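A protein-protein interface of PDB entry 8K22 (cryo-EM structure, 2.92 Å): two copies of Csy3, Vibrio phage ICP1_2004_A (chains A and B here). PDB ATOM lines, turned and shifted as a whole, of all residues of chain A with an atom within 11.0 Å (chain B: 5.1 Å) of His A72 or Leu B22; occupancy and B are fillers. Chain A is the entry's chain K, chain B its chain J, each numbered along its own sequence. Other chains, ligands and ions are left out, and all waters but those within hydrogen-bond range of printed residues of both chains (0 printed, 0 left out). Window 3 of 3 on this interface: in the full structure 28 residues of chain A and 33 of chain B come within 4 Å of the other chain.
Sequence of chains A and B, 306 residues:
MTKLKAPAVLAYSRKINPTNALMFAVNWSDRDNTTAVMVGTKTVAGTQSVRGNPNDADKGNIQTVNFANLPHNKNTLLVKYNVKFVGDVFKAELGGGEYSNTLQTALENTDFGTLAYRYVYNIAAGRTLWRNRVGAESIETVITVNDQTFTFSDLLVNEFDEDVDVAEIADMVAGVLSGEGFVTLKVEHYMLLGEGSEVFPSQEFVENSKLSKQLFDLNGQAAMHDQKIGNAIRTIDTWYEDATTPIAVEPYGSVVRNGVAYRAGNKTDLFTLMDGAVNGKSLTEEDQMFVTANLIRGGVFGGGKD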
ATOM      1  N   ALA A  25       1.447  -3.016  21.829  1.00  0.00           N
ATOM      2  CA  ALA A  25       0.766  -1.934  21.132  1.00  0.00           C
ATOM      3  C   ALA A  25      -0.694  -1.926  21.553  1.00  0.00           C
ATOM      4  O   ALA A  25      -1.392  -2.934  21.404  1.00  0.00           O
ATOM      5  CB  ALA A  25       0.891  -2.095  19.621  1.00  0.00           C
ATOM      6  N   VAL A  26      -1.152  -0.794  22.077  1.00  0.00           N
ATOM      7  CA  VAL A  26      -2.520  -0.621  22.521  1.00  0.00           C
ATOM      8  C   VAL A  26      -3.040   0.702  21.974  1.00  0.00           C
ATOM      9  O   VAL A  26      -2.295   1.502  21.417  1.00  0.00           O
ATOM     10  CB  VAL A  26      -2.646  -0.656  24.056  1.00  0.00           C
ATOM     11  CG1 VAL A  26      -2.561  -2.067  24.559  1.00  0.00           C
ATOM     12  CG2 VAL A  26      -1.571   0.198  24.689  1.00  0.00           C
ATOM     13  N   ASN A  27      -4.334   0.922  22.146  1.00  0.00           N
ATOM     14  CA  ASN A  27      -4.945   2.212  21.883  1.00  0.00           C
ATOM     15  C   ASN A  27      -5.169   2.937  23.201  1.00  0.00           C
ATOM     16  O   ASN A  27      -5.255   2.328  24.269  1.00  0.00           O
ATOM     17  CB  ASN A  27      -6.265   2.047  21.124  1.00  0.00           C
ATOM     18  CG  ASN A  27      -6.068   1.998  19.626  1.00  0.00           C
ATOM     19  OD1 ASN A  27      -6.550   1.090  18.954  1.00  0.00           O
ATOM     20  ND2 ASN A  27      -5.365   2.989  19.093  1.00  0.00           N
ATOM     21  N   ASP A  30      -8.668   1.538  23.895  1.00  0.00           N
ATOM     22  CA  ASP A  30      -8.592   0.168  24.380  1.00  0.00           C
ATOM     23  C   ASP A  30      -7.175  -0.175  24.791  1.00  0.00           C
ATOM     24  O   ASP A  30      -6.385  -0.670  23.988  1.00  0.00           O
ATOM     25  CB  ASP A  30      -9.124  -0.832  23.348  1.00  0.00           C
ATOM     26  CG  ASP A  30      -8.979  -0.345  21.919  1.00  0.00           C
ATOM     27  OD1 ASP A  30      -9.805   0.479  21.475  1.00  0.00           O
ATOM     28  OD2 ASP A  30      -8.042  -0.802  21.232  1.00  0.00           O
ATOM     29  N   THR A  35      -0.866  -5.936  21.969  1.00  0.00           N
ATOM     30  CA  THR A  35      -0.390  -6.617  20.770  1.00  0.00           C
ATOM     31  C   THR A  35       1.118  -6.517  20.673  1.00  0.00           C
ATOM     32  O   THR A  35       1.658  -5.429  20.508  1.00  0.00           O
ATOM     33  CB  THR A  35      -1.040  -6.049  19.493  1.00  0.00           C
ATOM     34  OG1 THR A  35      -2.452  -6.289  19.535  1.00  0.00           O
ATOM     35  CG2 THR A  35      -0.470  -6.709  18.244  1.00  0.00           C
ATOM     36  N   ALA A  36       1.800  -7.649  20.782  1.00  0.00           N
ATOM     37  CA  ALA A  36       3.258  -7.669  20.717  1.00  0.00           C
ATOM     38  C   ALA A  36       3.847  -6.818  19.603  1.00  0.00           C
ATOM     39  O   ALA A  36       3.664  -7.132  18.428  1.00  0.00           O
ATOM     40  CB  ALA A  36       3.725  -9.105  20.559  1.00  0.00           C
ATOM     41  N   VAL A  37       4.544  -5.740  19.955  1.00  0.00           N
ATOM     42  CA  VAL A  37       5.216  -4.947  18.929  1.00  0.00           C
ATOM     43  C   VAL A  37       6.308  -5.850  18.403  1.00  0.00           C
ATOM     44  O   VAL A  37       7.187  -6.248  19.150  1.00  0.00           O
ATOM     45  CB  VAL A  37       5.844  -3.659  19.494  1.00  0.00           C
ATOM     46  CG1 VAL A  37       6.719  -2.980  18.448  1.00  0.00           C
ATOM     47  CG2 VAL A  37       4.765  -2.701  19.954  1.00  0.00           C
ATOM     48  N   MET A  38       6.249  -6.208  17.129  1.00  0.00           N
ATOM     49  CA  MET A  38       7.224  -7.148  16.601  1.00  0.00           C
ATOM     50  C   MET A  38       8.495  -6.473  16.124  1.00  0.00           C
ATOM     51  O   MET A  38       8.435  -5.417  15.490  1.00  0.00           O
ATOM     52  CB  MET A  38       6.615  -7.949  15.452  1.00  0.00           C
ATOM     53  CG  MET A  38       5.538  -8.922  15.891  1.00  0.00           C
ATOM     54  SD  MET A  38       5.990  -9.781  17.408  1.00  0.00           S
ATOM     55  CE  MET A  38       6.489 -11.368  16.750  1.00  0.00           C
ATOM     56  N   PHE A  67      14.245  -2.765  13.217  1.00  0.00           N
ATOM     57  CA  PHE A  67      13.407  -1.651  13.626  1.00  0.00           C
ATOM     58  C   PHE A  67      12.254  -2.183  14.461  1.00  0.00           C
ATOM     59  O   PHE A  67      11.975  -3.383  14.482  1.00  0.00           O
ATOM     60  CB  PHE A  67      12.858  -0.857  12.426  1.00  0.00           C
ATOM     61  CG  PHE A  67      11.752  -1.556  11.671  1.00  0.00           C
ATOM     62  CD1 PHE A  67      12.035  -2.579  10.785  1.00  0.00           C
ATOM     63  CD2 PHE A  67      10.431  -1.164  11.827  1.00  0.00           C
ATOM     64  CE1 PHE A  67      11.026  -3.207  10.082  1.00  0.00           C
ATOM     65  CE2 PHE A  67       9.419  -1.794  11.136  1.00  0.00           C
ATOM     66  CZ  PHE A  67       9.717  -2.816  10.261  1.00  0.00           C
ATOM     67  N   ALA A  68      11.580  -1.268  15.147  1.00  0.00           N
ATOM     68  CA  ALA A  68      10.377  -1.599  15.905  1.00  0.00           C
ATOM     69  C   ALA A  68       9.454  -0.394  15.864  1.00  0.00           C
ATOM     70  O   ALA A  68       9.759   0.647  16.451  1.00  0.00           O
ATOM     71  CB  ALA A  68      10.712  -1.986  17.341  1.00  0.00           C
ATOM     72  N   ASN A  69       8.329  -0.535  15.174  1.00  0.00           N
ATOM     73  CA  ASN A  69       7.346   0.524  15.036  1.00  0.00           C
ATOM     74  C   ASN A  69       6.003   0.048  15.564  1.00  0.00           C
ATOM     75  O   ASN A  69       5.723  -1.152  15.615  1.00  0.00           O
ATOM     76  CB  ASN A  69       7.196   0.962  13.574  1.00  0.00           C
ATOM     77  CG  ASN A  69       8.276   1.925  13.140  1.00  0.00           C
ATOM     78  OD1 ASN A  69       9.460   1.594  13.146  1.00  0.00           O
ATOM     79  ND2 ASN A  69       7.872   3.125  12.747  1.00  0.00           N
ATOM     80  N   LEU A  70       5.180   1.004  15.971  1.00  0.00           N
ATOM     81  CA  LEU A  70       3.801   0.687  16.289  1.00  0.00           C
ATOM     82  C   LEU A  70       3.048   0.330  15.012  1.00  0.00           C
ATOM     83  O   LEU A  70       3.348   0.872  13.943  1.00  0.00           O
ATOM     84  CB  LEU A  70       3.115   1.864  16.976  1.00  0.00           C
ATOM     85  CG  LEU A  70       3.490   2.140  18.428  1.00  0.00           C
ATOM     86  CD1 LEU A  70       2.718   3.329  18.961  1.00  0.00           C
ATOM     87  CD2 LEU A  70       3.241   0.912  19.279  1.00  0.00           C
ATOM     88  N   PRO A  71       2.098  -0.595  15.081  1.00  0.00           N
ATOM     89  CA  PRO A  71       1.183  -0.789  13.955  1.00  0.00           C
ATOM     90  C   PRO A  71       0.290   0.426  13.777  1.00  0.00           C
ATOM     91  O   PRO A  71       0.040   1.185  14.715  1.00  0.00           O
ATOM     92  CB  PRO A  71       0.376  -2.026  14.359  1.00  0.00           C
ATOM     93  CG  PRO A  71       0.550  -2.134  15.836  1.00  0.00           C
ATOM     94  CD  PRO A  71       1.919  -1.620  16.116  1.00  0.00           C
ATOM     95  N   HIS A  72      -0.198   0.605  12.553  1.00  0.00           N
ATOM     96  CA  HIS A  72      -0.918   1.819  12.194  1.00  0.00           C
ATOM     97  C   HIS A  72      -2.379   1.823  12.631  1.00  0.00           C
ATOM     98  O   HIS A  72      -3.128   2.705  12.200  1.00  0.00           O
ATOM     99  CB  HIS A  72      -0.832   2.048  10.686  1.00  0.00           C
ATOM    100  CG  HIS A  72       0.343   2.878  10.273  1.00  0.00           C
ATOM    101  ND1 HIS A  72       1.594   2.343  10.060  1.00  0.00           N
ATOM    102  CD2 HIS A  72       0.456   4.207  10.039  1.00  0.00           C
ATOM    103  CE1 HIS A  72       2.428   3.306   9.709  1.00  0.00           C
ATOM    104  NE2 HIS A  72       1.762   4.446   9.688  1.00  0.00           N
ATOM    105  N   ASN A  73      -2.808   0.877  13.462  1.00  0.00           N
ATOM    106  CA  ASN A  73      -4.129   0.932  14.068  1.00  0.00           C
ATOM    107  C   ASN A  73      -4.074   1.159  15.571  1.00  0.00           C
ATOM    108  O   ASN A  73      -5.124   1.362  16.190  1.00  0.00           O
ATOM    109  CB  ASN A  73      -4.909  -0.350  13.769  1.00  0.00           C
ATOM    110  CG  ASN A  73      -4.053  -1.585  13.880  1.00  0.00           C
ATOM    111  OD1 ASN A  73      -2.857  -1.496  14.139  1.00  0.00           O
ATOM    112  ND2 ASN A  73      -4.660  -2.749  13.688  1.00  0.00           N
ATOM    113  N   LYS A  74      -2.885   1.129  16.175  1.00  0.00           N
ATOM    114  CA  LYS A  74      -2.714   1.415  17.595  1.00  0.00           C
ATOM    115  C   LYS A  74      -1.731   2.561  17.767  1.00  0.00           C
ATOM    116  O   LYS A  74      -0.642   2.544  17.185  1.00  0.00           O
ATOM    117  CB  LYS A  74      -2.242   0.182  18.375  1.00  0.00           C
ATOM    118  CG  LYS A  74      -2.824  -1.127  17.884  1.00  0.00           C
ATOM    119  CD  LYS A  74      -4.155  -1.381  18.572  1.00  0.00           C
ATOM    120  CE  LYS A  74      -4.547  -2.841  18.545  1.00  0.00           C
ATOM    121  NZ  LYS A  74      -3.573  -3.671  19.294  1.00  0.00           N
ATOM    122  N   ASN A  75      -2.115   3.547  18.575  1.00  0.00           N
ATOM    123  CA  ASN A  75      -1.353   4.778  18.742  1.00  0.00           C
ATOM    124  C   ASN A  75      -0.644   4.863  20.085  1.00  0.00           C
ATOM    125  O   ASN A  75      -0.099   5.919  20.419  1.00  0.00           O
ATOM    126  CB  ASN A  75      -2.269   5.991  18.566  1.00  0.00           C
ATOM    127  CG  ASN A  75      -3.597   5.832  19.282  1.00  0.00           C
ATOM    128  OD1 ASN A  75      -3.774   4.928  20.096  1.00  0.00           O
ATOM    129  ND2 ASN A  75      -4.542   6.714  18.978  1.00  0.00           N
ATOM    130  N   THR A  76      -0.636   3.785  20.861  1.00  0.00           N
ATOM    131  CA  THR A  76      -0.099   3.800  22.213  1.00  0.00           C
ATOM    132  C   THR A  76       0.891   2.659  22.380  1.00  0.00           C
ATOM    133  O   THR A  76       0.596   1.517  22.012  1.00  0.00           O
ATOM    134  CB  THR A  76      -1.224   3.680  23.247  1.00  0.00           C
ATOM    135  OG1 THR A  76      -2.227   4.665  22.976  1.00  0.00           O
ATOM    136  CG2 THR A  76      -0.692   3.895  24.654  1.00  0.00           C
ATOM    137  N   LEU A  77       2.057   2.969  22.934  1.00  0.00           N
ATOM    138  CA  LEU A  77       3.038   1.961  23.307  1.00  0.00           C
ATOM    139  C   LEU A  77       2.855   1.596  24.773  1.00  0.00           C
ATOM    140  O   LEU A  77       2.892   2.467  25.647  1.00  0.00           O
ATOM    141  CB  LEU A  77       4.459   2.464  23.061  1.00  0.00           C
ATOM    142  CG  LEU A  77       5.556   1.546  23.598  1.00  0.00           C
ATOM    143  CD1 LEU A  77       5.597   0.245  22.827  1.00  0.00           C
ATOM    144  CD2 LEU A  77       6.898   2.242  23.542  1.00  0.00           C
ATOM    145  N   LEU A 193       2.220   7.681  21.791  1.00  0.00           N
ATOM    146  CA  LEU A 193       3.214   8.094  20.810  1.00  0.00           C
ATOM    147  C   LEU A 193       2.568   8.570  19.517  1.00  0.00           C
ATOM    148  O   LEU A 193       3.037   9.537  18.907  1.00  0.00           O
ATOM    149  CB  LEU A 193       4.180   6.947  20.531  1.00  0.00           C
ATOM    150  CG  LEU A 193       5.309   6.805  21.543  1.00  0.00           C
ATOM    151  CD1 LEU A 193       6.085   5.527  21.301  1.00  0.00           C
ATOM    152  CD2 LEU A 193       6.214   8.011  21.433  1.00  0.00           C
ATOM    153  N   GLY A 194       1.505   7.911  19.085  1.00  0.00           N
ATOM    154  CA  GLY A 194       0.839   8.245  17.846  1.00  0.00           C
ATOM    155  C   GLY A 194       0.765   7.058  16.903  1.00  0.00           C
ATOM    156  O   GLY A 194       1.295   5.980  17.160  1.00  0.00           O
ATOM    157  N   GLU A 195       0.094   7.300  15.782  1.00  0.00           N
ATOM    158  CA  GLU A 195      -0.204   6.246  14.823  1.00  0.00           C
ATOM    159  C   GLU A 195       1.060   5.837  14.080  1.00  0.00           C
ATOM    160  O   GLU A 195       1.620   6.625  13.312  1.00  0.00           O
ATOM    161  CB  GLU A 195      -1.265   6.729  13.839  1.00  0.00           C
ATOM    162  CG  GLU A 195      -2.257   5.668  13.435  1.00  0.00           C
ATOM    163  CD  GLU A 195      -3.125   5.235  14.592  1.00  0.00           C
ATOM    164  OE1 GLU A 195      -3.856   6.087  15.139  1.00  0.00           O
ATOM    165  OE2 GLU A 195      -3.069   4.046  14.964  1.00  0.00           O
ATOM    166  N   GLY A 196       1.509   4.606  14.307  1.00  0.00           N
ATOM    167  CA  GLY A 196       2.671   4.097  13.611  1.00  0.00           C
ATOM    168  C   GLY A 196       3.985   4.701  14.034  1.00  0.00           C
ATOM    169  O   GLY A 196       4.948   4.659  13.263  1.00  0.00           O
ATOM    170  N   SER A 197       4.053   5.275  15.232  1.00  0.00           N
ATOM    171  CA  SER A 197       5.290   5.875  15.708  1.00  0.00           C
ATOM    172  C   SER A 197       6.300   4.795  16.065  1.00  0.00           C
ATOM    173  O   SER A 197       5.945   3.741  16.597  1.00  0.00           O
ATOM    174  CB  SER A 197       5.018   6.758  16.920  1.00  0.00           C
ATOM    175  OG  SER A 197       6.205   7.389  17.363  1.00  0.00           O
ATOM    176  N   GLU A 198       7.564   5.061  15.758  1.00  0.00           N
ATOM    177  CA  GLU A 198       8.621   4.094  16.006  1.00  0.00           C
ATOM    178  C   GLU A 198       8.934   4.044  17.495  1.00  0.00           C
ATOM    179  O   GLU A 198       9.116   5.083  18.136  1.00  0.00           O
ATOM    180  CB  GLU A 198       9.867   4.455  15.194  1.00  0.00           C
ATOM    181  CG  GLU A 198      11.197   4.064  15.817  1.00  0.00           C
ATOM    182  CD  GLU A 198      12.344   4.171  14.833  1.00  0.00           C
ATOM    183  OE1 GLU A 198      12.156   3.791  13.659  1.00  0.00           O
ATOM    184  OE2 GLU A 198      13.433   4.634  15.229  1.00  0.00           O
ATOM    185  N   VAL A 199       8.968   2.837  18.045  1.00  0.00           N
ATOM    186  CA  VAL A 199       9.299   2.638  19.441  1.00  0.00           C
ATOM    187  C   VAL A 199      10.766   2.255  19.532  1.00  0.00           C
ATOM    188  O   VAL A 199      11.407   1.883  18.547  1.00  0.00           O
ATOM    189  CB  VAL A 199       8.395   1.581  20.109  1.00  0.00           C
ATOM    190  CG1 VAL A 199       6.961   1.823  19.728  1.00  0.00           C
ATOM    191  CG2 VAL A 199       8.815   0.184  19.716  1.00  0.00           C
ATOM    192  N   THR B  19       6.586   8.885  10.304  1.00  0.00           N
ATOM    193  CA  THR B  19       6.149   7.503  10.315  1.00  0.00           C
ATOM    194  C   THR B  19       6.166   6.961   8.892  1.00  0.00           C
ATOM    195  O   THR B  19       6.461   7.677   7.933  1.00  0.00           O
ATOM    196  CB  THR B  19       4.762   7.383  10.939  1.00  0.00           C
ATOM    197  OG1 THR B  19       3.815   8.088  10.132  1.00  0.00           O
ATOM    198  CG2 THR B  19       4.761   7.965  12.340  1.00  0.00           C
ATOM    199  N   ASN B  20       5.859   5.677   8.746  1.00  0.00           N
ATOM    200  CA  ASN B  20       5.735   5.097   7.419  1.00  0.00           C
ATOM    201  C   ASN B  20       4.456   5.600   6.767  1.00  0.00           C
ATOM    202  O   ASN B  20       3.374   5.520   7.353  1.00  0.00           O
ATOM    203  CB  ASN B  20       5.738   3.575   7.502  1.00  0.00           C
ATOM    204  CG  ASN B  20       7.041   3.028   8.037  1.00  0.00           C
ATOM    205  OD1 ASN B  20       8.118   3.451   7.622  1.00  0.00           O
ATOM    206  ND2 ASN B  20       6.952   2.083   8.961  1.00  0.00           N
ATOM    207  N   ALA B  21       4.582   6.126   5.556  1.00  0.00           N
ATOM    208  CA  ALA B  21       3.498   6.861   4.914  1.00  0.00           C
ATOM    209  C   ALA B  21       2.608   5.890   4.162  1.00  0.00           C
ATOM    210  O   ALA B  21       2.919   5.495   3.039  1.00  0.00           O
ATOM    211  CB  ALA B  21       4.057   7.916   3.972  1.00  0.00           C
ATOM    212  N   LEU B  22       1.483   5.525   4.768  1.00  0.00           N
ATOM    213  CA  LEU B  22       0.539   4.634   4.110  1.00  0.00           C
ATOM    214  C   LEU B  22      -0.155   5.354   2.964  1.00  0.00           C
ATOM    215  O   LEU B  22      -0.602   6.492   3.113  1.00  0.00           O
ATOM    216  CB  LEU B  22      -0.503   4.134   5.105  1.00  0.00           C
ATOM    217  CG  LEU B  22      -0.031   3.190   6.202  1.00  0.00           C
ATOM    218  CD1 LEU B  22      -1.217   2.750   7.035  1.00  0.00           C
ATOM    219  CD2 LEU B  22       0.676   1.997   5.601  1.00  0.00           C
ATOM    220  N   MET B  23      -0.256   4.692   1.818  1.00  0.00           N
ATOM    221  CA  MET B  23      -0.999   5.247   0.697  1.00  0.00           C
ATOM    222  C   MET B  23      -2.368   4.600   0.573  1.00  0.00           C
ATOM    223  O   MET B  23      -2.492   3.372   0.534  1.00  0.00           O
ATOM    224  CB  MET B  23      -0.232   5.119  -0.611  1.00  0.00           C
ATOM    225  CG  MET B  23       1.234   5.326  -0.492  1.00  0.00           C
ATOM    226  SD  MET B  23       2.040   4.832  -2.004  1.00  0.00           S
ATOM    227  CE  MET B  23       3.511   5.806  -1.819  1.00  0.00           C
ATOM    228  N   PHE B  24      -3.384   5.446   0.517  1.00  0.00           N
ATOM    229  CA  PHE B  24      -4.764   5.092   0.262  1.00  0.00           C
ATOM    230  C   PHE B  24      -5.175   5.654  -1.092  1.00  0.00           C
ATOM    231  O   PHE B  24      -4.454   6.442  -1.710  1.00  0.00           O
ATOM    232  CB  PHE B  24      -5.684   5.644   1.357  1.00  0.00           C
ATOM    233  CG  PHE B  24      -5.433   5.060   2.719  1.00  0.00           C
ATOM    234  CD1 PHE B  24      -4.477   5.614   3.560  1.00  0.00           C
ATOM    235  CD2 PHE B  24      -6.157   3.966   3.163  1.00  0.00           C
ATOM    236  CE1 PHE B  24      -4.242   5.083   4.810  1.00  0.00           C
ATOM    237  CE2 PHE B  24      -5.930   3.430   4.418  1.00  0.00           C
ATOM    238  CZ  PHE B  24      -4.970   3.992   5.243  1.00  0.00           C
ATOM    239  N   LEU B  78      -3.734   9.250  -1.929  1.00  0.00           N
ATOM    240  CA  LEU B  78      -3.584   9.837  -0.607  1.00  0.00           C
ATOM    241  C   LEU B  78      -2.393   9.212   0.100  1.00  0.00           C
ATOM    242  O   LEU B  78      -2.226   7.994   0.088  1.00  0.00           O
ATOM    243  CB  LEU B  78      -4.863   9.656   0.209  1.00  0.00           C
ATOM    244  CG  LEU B  78      -4.837   9.737   1.732  1.00  0.00           C
ATOM    245  CD1 LEU B  78      -4.400  11.090   2.251  1.00  0.00           C
ATOM    246  CD2 LEU B  78      -6.241   9.436   2.191  1.00  0.00           C
ATOM    247  N   VAL B  79      -1.568  10.058   0.701  1.00  0.00           N
ATOM    248  CA  VAL B  79      -0.391   9.635   1.450  1.00  0.00           C
ATOM    249  C   VAL B  79      -0.531  10.165   2.873  1.00  0.00           C
ATOM    250  O   VAL B  79      -0.613  11.381   3.078  1.00  0.00           O
ATOM    251  CB  VAL B  79       0.902  10.129   0.781  1.00  0.00           C
ATOM    252  CG1 VAL B  79       2.068  10.029   1.720  1.00  0.00           C
ATOM    253  CG2 VAL B  79       1.178   9.330  -0.481  1.00  0.00           C
ATOM    254  N   LYS B  80      -0.578   9.260   3.848  1.00  0.00           N
ATOM    255  CA  LYS B  80      -0.668   9.612   5.261  1.00  0.00           C
ATOM    256  C   LYS B  80       0.661   9.338   5.937  1.00  0.00           C
ATOM    257  O   LYS B  80       1.240   8.259   5.759  1.00  0.00           O
ATOM    258  CB  LYS B  80      -1.762   8.823   5.986  1.00  0.00           C
ATOM    259  CG  LYS B  80      -2.726   9.677   6.798  1.00  0.00           C
ATOM    260  CD  LYS B  80      -3.921   8.874   7.291  1.00  0.00           C
ATOM    261  CE  LYS B  80      -4.807   8.455   6.156  1.00  0.00           C
ATOM    262  NZ  LYS B  80      -4.976   9.615   5.259  1.00  0.00           N
ATOM    263  N   LEU B 218       2.989  -2.386   4.225  1.00  0.00           N
ATOM    264  CA  LEU B 218       2.581  -2.567   5.612  1.00  0.00           C
ATOM    265  C   LEU B 218       1.248  -3.299   5.596  1.00  0.00           C
ATOM    266  O   LEU B 218       0.214  -2.696   5.288  1.00  0.00           O
ATOM    267  CB  LEU B 218       2.471  -1.230   6.338  1.00  0.00           C
ATOM    268  CG  LEU B 218       3.791  -0.590   6.763  1.00  0.00           C
ATOM    269  CD1 LEU B 218       3.514   0.591   7.662  1.00  0.00           C
ATOM    270  CD2 LEU B 218       4.688  -1.596   7.462  1.00  0.00           C
ATOM    271  N   GLN B 221      -0.512  -3.117   2.225  1.00  0.00           N
ATOM    272  CA  GLN B 221      -0.792  -1.779   1.725  1.00  0.00           C
ATOM    273  C   GLN B 221       0.498  -1.070   1.344  1.00  0.00           C
ATOM    274  O   GLN B 221       1.482  -1.116   2.082  1.00  0.00           O
ATOM    275  CB  GLN B 221      -1.545  -0.969   2.781  1.00  0.00           C
ATOM    276  CG  GLN B 221      -1.757   0.487   2.416  1.00  0.00           C
ATOM    277  CD  GLN B 221      -2.510   1.248   3.473  1.00  0.00           C
ATOM    278  OE1 GLN B 221      -2.667   0.781   4.599  1.00  0.00           O
ATOM    279  NE2 GLN B 221      -2.984   2.434   3.119  1.00  0.00           N
ATOM    280  N   ALA B 222       0.491  -0.430   0.172  1.00  0.00           N
ATOM    281  CA  ALA B 222       1.651   0.308  -0.309  1.00  0.00           C
ATOM    282  C   ALA B 222       1.987   1.469   0.617  1.00  0.00           C
ATOM    283  O   ALA B 222       1.116   2.252   1.005  1.00  0.00           O
ATOM    284  CB  ALA B 222       1.395   0.825  -1.722  1.00  0.00           C
ATOM    285  N   ALA B 223       3.264   1.572   0.971  1.00  0.00           N
ATOM    286  CA  ALA B 223       3.703   2.534   1.965  1.00  0.00           C
ATOM    287  C   ALA B 223       5.082   3.056   1.601  1.00  0.00           C
ATOM    288  O   ALA B 223       5.819   2.439   0.831  1.00  0.00           O
ATOM    289  CB  ALA B 223       3.727   1.925   3.369  1.00  0.00           C
ATOM    290  N   MET B 224       5.463   4.166   2.234  1.00  0.00           N
ATOM    291  CA  MET B 224       6.787   4.741   2.004  1.00  0.00           C
ATOM    292  C   MET B 224       7.654   4.656   3.253  1.00  0.00           C
ATOM    293  O   MET B 224       7.162   4.853   4.359  1.00  0.00           O
ATOM    294  CB  MET B 224       6.669   6.194   1.550  1.00  0.00           C
ATOM    295  CG  MET B 224       6.915   6.395   0.067  1.00  0.00           C
ATOM    296  SD  MET B 224       7.152   8.124  -0.374  1.00  0.00           S
ATOM    297  CE  MET B 224       5.544   8.791   0.045  1.00  0.00           C
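NE2 of His A72 is in hydrogen-bond range of O of Asn B20.
The backbone carbonyl oxygen (O) of Leu B22 lies within hydrogen-bond range of the backbone NH (N) of Lys B80 (2.9 Å). The backbone NH of Lys A74 is in hydrogen-bond range of the side-chain carboxylate of Glu A195 (3.2 Å). The backbone carbonyl oxygen (O) of Ser A197 is in hydrogen-bond range of the backbone NH (N) of Leu A70, 2.9 Å away. The backbone carbonyl oxygen of Gly A196 sits at hydrogen-bond distance from the side-chain amide nitrogen of Asn A69, 3.3 Å away.
Leu B22 touches His A72 (CD1 to CG, 3.6 Å). ND1 of His A72 touches CD1 of Leu B218, 3.5 Å away. Glu A195 touches Thr B19 (O to CG2, 3.6 Å). Gly A196 touches Thr B19. CA of Ser A197 touches CG2 of Thr B19, at 3.999 Å.
Of chain B, only Asn B20, Leu B22 and Leu B218 come within 4 Å of His A72. Thr A76 touches none of the printed residues of chain B. Of the printed residues of chain B, Glu A195 touches Thr B19. Of the printed residues of chain A, Thr B19 touches Glu A195, Gly A196 and Ser A197. Asn B20 touches just one residue of chain A: His A72. Of chain A, only His A72 (3.6 Å) comes within 4 Å of Leu B22. No residue of chain A comes within 4 Å of Leu B78. No residue of chain A comes within 4 Å of Val B79. No residue of chain A comes within 4 Å of Lys B80. Leu B218 touches one residue of chain A. No residue of chain A comes within 4 Å of Gln B221. No residue of chain A comes within 4 Å of Ala B223. The nearest residue of chain B that does not touch His A72 is Thr B19 (4.2 Å).
Hydrophobic or aromatic side chains of chain B that line the printed part of chain A: Leu B22 and Leu B218. Hydrophobic or aromatic side chains of chain A within 4 Å of the printed part of chain B: His A72. Among the printed residues, 6 pairs touch across the chains. Among the printed residues, no Asp or Glu carboxylate lies within 4 Å of a Lys or Arg side-chain nitrogen of the other chain.
No position is printed for both chains. Of the 6 pairs that touch across the chains among the printed residues, none has its exchanged pair printed and touching as well.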
